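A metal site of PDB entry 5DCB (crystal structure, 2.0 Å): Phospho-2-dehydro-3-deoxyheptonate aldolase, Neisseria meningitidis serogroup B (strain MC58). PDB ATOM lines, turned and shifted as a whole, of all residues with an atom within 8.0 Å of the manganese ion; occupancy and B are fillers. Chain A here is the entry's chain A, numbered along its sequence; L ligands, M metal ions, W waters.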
ATOM      1  N   GLY A  61     -14.999  -1.456   8.136  1.00  0.00           N
ATOM      2  CA  GLY A  61     -16.402  -1.802   8.050  1.00  0.00           C
ATOM      3  C   GLY A  61     -16.973  -2.157   9.410  1.00  0.00           C
ATOM      4  O   GLY A  61     -16.320  -1.904  10.432  1.00  0.00           O
ATOM      5  N   PRO A  62     -18.200  -2.721   9.446  1.00  0.00           N
ATOM      6  CA  PRO A  62     -18.881  -2.867  10.715  1.00  0.00           C
ATOM      7  C   PRO A  62     -18.162  -3.795  11.698  1.00  0.00           C
ATOM      8  O   PRO A  62     -17.409  -4.678  11.295  1.00  0.00           O
ATOM      9  CB  PRO A  62     -20.214  -3.487  10.317  1.00  0.00           C
ATOM     10  CG  PRO A  62     -20.470  -3.004   8.926  1.00  0.00           C
ATOM     11  CD  PRO A  62     -19.113  -2.837   8.300  1.00  0.00           C
ATOM     12  N   CYS A  63     -18.404  -3.597  12.987  1.00  0.00           N
ATOM     13  CA  CYS A  63     -17.893  -4.527  13.963  1.00  0.00           C
ATOM     14  C   CYS A  63     -18.377  -5.926  13.621  1.00  0.00           C
ATOM     15  O   CYS A  63     -17.600  -6.870  13.589  1.00  0.00           O
ATOM     16  CB  CYS A  63     -18.356  -4.136  15.360  1.00  0.00           C
ATOM     17  SG  CYS A  63     -18.003  -5.382  16.634  1.00  0.00           S
ATOM     18  N   SER A  64     -19.675  -6.025  13.321  1.00  0.00           N
ATOM     19  CA  SER A  64     -20.313  -7.258  12.938  1.00  0.00           C
ATOM     20  C   SER A  64     -21.404  -6.957  11.937  1.00  0.00           C
ATOM     21  O   SER A  64     -21.993  -5.854  11.952  1.00  0.00           O
ATOM     22  CB  SER A  64     -20.898  -7.974  14.157  1.00  0.00           C
ATOM     23  OG  SER A  64     -21.975  -7.242  14.740  1.00  0.00           O
ATOM     24  N   ARG A  94     -14.499  -4.993   5.990  1.00  0.00           N
ATOM     25  CA  ARG A  94     -14.612  -5.844   7.161  1.00  0.00           C
ATOM     26  C   ARG A  94     -15.981  -6.514   7.154  1.00  0.00           C
ATOM     27  O   ARG A  94     -16.987  -5.835   7.291  1.00  0.00           O
ATOM     28  CB  ARG A  94     -14.473  -4.968   8.405  1.00  0.00           C
ATOM     29  CG  ARG A  94     -14.324  -5.718   9.706  1.00  0.00           C
ATOM     30  CD  ARG A  94     -14.137  -4.783  10.912  1.00  0.00           C
ATOM     31  NE  ARG A  94     -14.712  -5.432  12.067  1.00  0.00           N
ATOM     32  CZ  ARG A  94     -14.041  -6.056  13.035  1.00  0.00           C
ATOM     33  NH1 ARG A  94     -12.712  -6.054  13.058  1.00  0.00           N
ATOM     34  NH2 ARG A  94     -14.732  -6.656  14.004  1.00  0.00           N
ATOM     35  N   TYR A  96     -17.352  -9.290   9.290  1.00  0.00           N
ATOM     36  CA  TYR A  96     -17.322 -10.217  10.414  1.00  0.00           C
ATOM     37  C   TYR A  96     -18.757 -10.501  10.799  1.00  0.00           C
ATOM     38  O   TYR A  96     -19.512  -9.571  11.024  1.00  0.00           O
ATOM     39  CB  TYR A  96     -16.578  -9.623  11.620  1.00  0.00           C
ATOM     40  CG  TYR A  96     -15.076  -9.460  11.430  1.00  0.00           C
ATOM     41  CD1 TYR A  96     -14.524  -9.211  10.187  1.00  0.00           C
ATOM     42  CD2 TYR A  96     -14.220  -9.515  12.521  1.00  0.00           C
ATOM     43  CE1 TYR A  96     -13.138  -9.044  10.028  1.00  0.00           C
ATOM     44  CE2 TYR A  96     -12.854  -9.335  12.360  1.00  0.00           C
ATOM     45  CZ  TYR A  96     -12.320  -9.114  11.123  1.00  0.00           C
ATOM     46  OH  TYR A  96     -10.963  -8.910  10.980  1.00  0.00           O
ATOM     47  N   GLU A  98     -19.749 -12.345  13.484  1.00  0.00           N
ATOM     48  CA  GLU A  98     -19.954 -12.609  14.898  1.00  0.00           C
ATOM     49  C   GLU A  98     -18.926 -11.878  15.736  1.00  0.00           C
ATOM     50  O   GLU A  98     -17.766 -11.748  15.337  1.00  0.00           O
ATOM     51  CB  GLU A  98     -19.852 -14.114  15.169  1.00  0.00           C
ATOM     52  CG  GLU A  98     -20.084 -14.484  16.635  1.00  0.00           C
ATOM     53  CD  GLU A  98     -19.943 -15.981  16.931  1.00  0.00           C
ATOM     54  OE1 GLU A  98     -19.997 -16.360  18.139  1.00  0.00           O
ATOM     55  OE2 GLU A  98     -19.827 -16.780  15.975  1.00  0.00           O
ATOM     56  N   LYS A  99     -19.324 -11.428  16.918  1.00  0.00           N
ATOM     57  CA  LYS A  99     -18.339 -10.981  17.868  1.00  0.00           C
ATOM     58  C   LYS A  99     -18.317 -11.964  19.010  1.00  0.00           C
ATOM     59  O   LYS A  99     -19.330 -12.166  19.681  1.00  0.00           O
ATOM     60  CB  LYS A  99     -18.652  -9.594  18.372  1.00  0.00           C
ATOM     61  CG  LYS A  99     -17.477  -8.954  19.074  1.00  0.00           C
ATOM     62  CD  LYS A  99     -17.994  -8.120  20.218  1.00  0.00           C
ATOM     63  CE  LYS A  99     -17.014  -7.055  20.647  1.00  0.00           C
ATOM     64  NZ  LYS A  99     -15.641  -7.500  20.962  1.00  0.00           N
ATOM     65  N   PRO A 100     -17.168 -12.586  19.235  1.00  0.00           N
ATOM     66  CA  PRO A 100     -17.014 -13.468  20.371  1.00  0.00           C
ATOM     67  C   PRO A 100     -17.329 -12.697  21.637  1.00  0.00           C
ATOM     68  O   PRO A 100     -17.023 -11.495  21.733  1.00  0.00           O
ATOM     69  CB  PRO A 100     -15.525 -13.827  20.344  1.00  0.00           C
ATOM     70  CG  PRO A 100     -15.110 -13.636  18.945  1.00  0.00           C
ATOM     71  CD  PRO A 100     -15.936 -12.513  18.420  1.00  0.00           C
ATOM     72  N   LYS A 188      -4.077 -11.194  15.791  1.00  0.00           N
ATOM     73  CA  LYS A 188      -4.148 -10.180  16.843  1.00  0.00           C
ATOM     74  C   LYS A 188      -3.299 -10.515  18.049  1.00  0.00           C
ATOM     75  O   LYS A 188      -3.177 -11.683  18.431  1.00  0.00           O
ATOM     76  CB  LYS A 188      -5.614  -9.952  17.257  1.00  0.00           C
ATOM     77  CG  LYS A 188      -6.433  -9.397  16.115  1.00  0.00           C
ATOM     78  CD  LYS A 188      -7.656  -8.624  16.553  1.00  0.00           C
ATOM     79  CE  LYS A 188      -7.800  -7.338  15.769  1.00  0.00           C
ATOM     80  NZ  LYS A 188      -8.890  -6.541  16.363  1.00  0.00           N
ATOM     81  N   ASP A 267      -4.836  -1.796  14.598  1.00  0.00           N
ATOM     82  CA  ASP A 267      -6.263  -1.611  14.784  1.00  0.00           C
ATOM     83  C   ASP A 267      -6.518  -0.309  15.530  1.00  0.00           C
ATOM     84  O   ASP A 267      -5.971  -0.104  16.622  1.00  0.00           O
ATOM     85  CB  ASP A 267      -6.807  -2.801  15.560  1.00  0.00           C
ATOM     86  CG  ASP A 267      -8.322  -2.795  15.731  1.00  0.00           C
ATOM     87  OD1 ASP A 267      -9.031  -1.865  15.273  1.00  0.00           O
ATOM     88  OD2 ASP A 267      -8.803  -3.756  16.352  1.00  0.00           O
ATOM     89  N   SER A 269      -9.381   0.514  16.594  1.00  0.00           N
ATOM     90  CA  SER A 269     -10.511   0.268  17.460  1.00  0.00           C
ATOM     91  C   SER A 269     -10.166  -0.627  18.675  1.00  0.00           C
ATOM     92  O   SER A 269      -9.012  -0.711  19.082  1.00  0.00           O
ATOM     93  CB  SER A 269     -11.646  -0.333  16.618  1.00  0.00           C
ATOM     94  OG  SER A 269     -12.880  -0.069  17.247  1.00  0.00           O
ATOM     95  N   HIS A 270     -11.194  -1.242  19.256  1.00  0.00           N
ATOM     96  CA  HIS A 270     -11.052  -2.141  20.403  1.00  0.00           C
ATOM     97  C   HIS A 270     -10.164  -1.555  21.510  1.00  0.00           C
ATOM     98  O   HIS A 270     -10.378  -0.411  21.887  1.00  0.00           O
ATOM     99  CB  HIS A 270     -10.625  -3.529  19.907  1.00  0.00           C
ATOM    100  CG  HIS A 270     -11.554  -4.076  18.865  1.00  0.00           C
ATOM    101  ND1 HIS A 270     -11.231  -4.096  17.527  1.00  0.00           N
ATOM    102  CD2 HIS A 270     -12.816  -4.554  18.956  1.00  0.00           C
ATOM    103  CE1 HIS A 270     -12.240  -4.604  16.837  1.00  0.00           C
ATOM    104  NE2 HIS A 270     -13.214  -4.880  17.674  1.00  0.00           N
ATOM    105  N   MET A 302      -6.821  -1.173  10.808  1.00  0.00           N
ATOM    106  CA  MET A 302      -8.193  -1.672  10.935  1.00  0.00           C
ATOM    107  C   MET A 302      -9.086  -0.621  11.569  1.00  0.00           C
ATOM    108  O   MET A 302      -8.718   0.028  12.554  1.00  0.00           O
ATOM    109  CB  MET A 302      -8.205  -2.933  11.777  1.00  0.00           C
ATOM    110  CG  MET A 302      -9.592  -3.551  11.932  1.00  0.00           C
ATOM    111  SD  MET A 302      -9.463  -5.080  12.878  1.00  0.00           S
ATOM    112  CE  MET A 302      -8.710  -6.143  11.643  1.00  0.00           C
ATOM    113  N   GLU A 304     -13.313   0.309  12.673  1.00  0.00           N
ATOM    114  CA  GLU A 304     -14.710  -0.140  12.860  1.00  0.00           C
ATOM    115  C   GLU A 304     -15.624   1.000  12.512  1.00  0.00           C
ATOM    116  O   GLU A 304     -15.668   2.013  13.198  1.00  0.00           O
ATOM    117  CB  GLU A 304     -14.966  -0.661  14.261  1.00  0.00           C
ATOM    118  CG  GLU A 304     -14.280  -1.983  14.536  1.00  0.00           C
ATOM    119  CD  GLU A 304     -14.740  -2.649  15.825  1.00  0.00           C
ATOM    120  OE1 GLU A 304     -14.624  -2.024  16.929  1.00  0.00           O
ATOM    121  OE2 GLU A 304     -15.203  -3.817  15.727  1.00  0.00           O
ATOM    122  N   SER A 321     -24.420  -0.355  14.401  1.00  0.00           N
ATOM    123  CA  SER A 321     -23.904  -1.556  15.064  1.00  0.00           C
ATOM    124  C   SER A 321     -24.716  -2.019  16.266  1.00  0.00           C
ATOM    125  O   SER A 321     -25.169  -1.181  17.085  1.00  0.00           O
ATOM    126  CB  SER A 321     -22.472  -1.294  15.528  1.00  0.00           C
ATOM    127  OG  SER A 321     -21.901  -2.461  16.084  1.00  0.00           O
ATOM    128  N   THR A 323     -23.125  -4.511  18.036  1.00  0.00           N
ATOM    129  CA  THR A 323     -21.976  -4.979  18.818  1.00  0.00           C
ATOM    130  C   THR A 323     -21.092  -3.748  19.165  1.00  0.00           C
ATOM    131  O   THR A 323     -21.613  -2.801  19.761  1.00  0.00           O
ATOM    132  CB  THR A 323     -21.245  -6.107  18.066  1.00  0.00           C
ATOM    133  OG1 THR A 323     -20.991  -5.695  16.711  1.00  0.00           O
ATOM    134  CG2 THR A 323     -22.099  -7.354  18.044  1.00  0.00           C
ATOM    135  N   ASP A 324     -19.814  -3.712  18.796  1.00  0.00           N
ATOM    136  CA  ASP A 324     -18.946  -2.589  19.186  1.00  0.00           C
ATOM    137  C   ASP A 324     -19.371  -1.335  18.419  1.00  0.00           C
ATOM    138  O   ASP A 324     -19.760  -1.403  17.245  1.00  0.00           O
ATOM    139  CB  ASP A 324     -17.467  -2.868  18.865  1.00  0.00           C
ATOM    140  CG  ASP A 324     -16.883  -4.006  19.669  1.00  0.00           C
ATOM    141  OD1 ASP A 324     -17.356  -4.253  20.782  1.00  0.00           O
ATOM    142  OD2 ASP A 324     -15.964  -4.683  19.196  1.00  0.00           O
ATOM    143  N   ALA A 325     -19.286  -0.181  19.092  1.00  0.00           N
ATOM    144  CA  ALA A 325     -19.623   1.101  18.497  1.00  0.00           C
ATOM    145  C   ALA A 325     -18.645   1.444  17.391  1.00  0.00           C
ATOM    146  O   ALA A 325     -17.468   1.234  17.516  1.00  0.00           O
ATOM    147  CB  ALA A 325     -19.621   2.202  19.569  1.00  0.00           C
ATOM    148  N   CYS A 326     -19.155   1.977  16.290  1.00  0.00           N
ATOM    149  CA  CYS A 326     -18.372   2.281  15.106  1.00  0.00           C
ATOM    150  C   CYS A 326     -18.502   3.741  14.814  1.00  0.00           C
ATOM    151  O   CYS A 326     -19.482   4.362  15.181  1.00  0.00           O
ATOM    152  CB  CYS A 326     -18.939   1.541  13.903  1.00  0.00           C
ATOM    153  SG  CYS A 326     -18.873  -0.261  14.016  1.00  0.00           S
HETATM  154  C1  LIG L   1     -10.517  -7.268  19.658  1.00  0.00           C
HETATM  155  O1  LIG L   1      -9.436  -6.886  19.165  1.00  0.00           O
HETATM  156  O2  LIG L   1     -10.715  -7.248  20.890  1.00  0.00           O
HETATM  157  C2  LIG L   1     -11.588  -7.724  18.766  1.00  0.00           C
HETATM  158  C3  LIG L   1     -12.655  -8.368  19.249  1.00  0.00           C
HETATM  159  O3  LIG L   1     -11.400  -7.413  17.351  1.00  0.00           O
HETATM  160  P1  LIG L   1     -11.893  -8.321  16.125  1.00  0.00           P
HETATM  161  O4  LIG L   1     -11.239  -7.608  14.959  1.00  0.00           O
HETATM  162  O5  LIG L   1     -11.302  -9.675  16.460  1.00  0.00           O
HETATM  163  O6  LIG L   1     -13.392  -8.176  16.164  1.00  0.00           O
HETATM  164 MN    MN M   1     -15.531  -5.046  17.274  1.00  0.00          MN
HETATM  165  O   HOH W   1     -15.278  -7.129  17.201  1.00  0.00           O
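An oxygen (O4) of the ligand lies within salt-bridge range of the guanidinium group (NH1) of Arg 94. A ring nitrogen (ND1) of His 270 sits close to an oxygen (O3) of the ligand (3.3 Å). NZ of Lys 188 lies within salt-bridge range of O1 of the ligand.
The side-chain sulfur of Cys 63 sits close to the side-chain hydroxyl of Thr 323 (3.0 Å). The side-chain amino group (NZ) of Lys 99 lies within salt-bridge range of the side-chain carboxylate (OD1) of Asp 324 (3.7 Å). The side-chain carboxylate (OE1) of Glu 304 lies within hydrogen-bond range of the side-chain hydroxyl (OG) of Ser 269, 2.6 Å away. NH2 of Arg 94 lies close to OE2 of Glu 304, at 3.4 Å. ND1 of His 270 is in hydrogen-bond range of OD2 of Asp 267, at 2.7 Å. NH1 of Arg 94 sits at hydrogen-bond distance from SD of Met 302, at 3.4 Å. The side-chain hydroxyl (OG) of Ser 321 is in hydrogen-bond range of the backbone carbonyl oxygen (O) of Asp 324, 2.7 Å away. The backbone carbonyl oxygen (O) of Asp 324 sits at hydrogen-bond distance from the side-chain sulfur (SG) of Cys 326 (3.5 Å).
Arg 94 touches the manganese ion (NH2 to MN, 3.7 Å). Within 4 Å of the manganese ion: Cys 63, Arg 94, His 270, Glu 304 and Asp 324. The nearest printed residue that does not touch the manganese ion is Lys 99 (4.2 Å).
The manganese ion is bound by the side-chain carboxylate of Glu 304 (2.0 Å), the side-chain carboxylate of Asp 324 (2.0 Å), water W1 (2.1 Å), a ring nitrogen (NE2) of His 270 (2.4 Å) and the side-chain sulfur of Cys 63 (2.6 Å).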
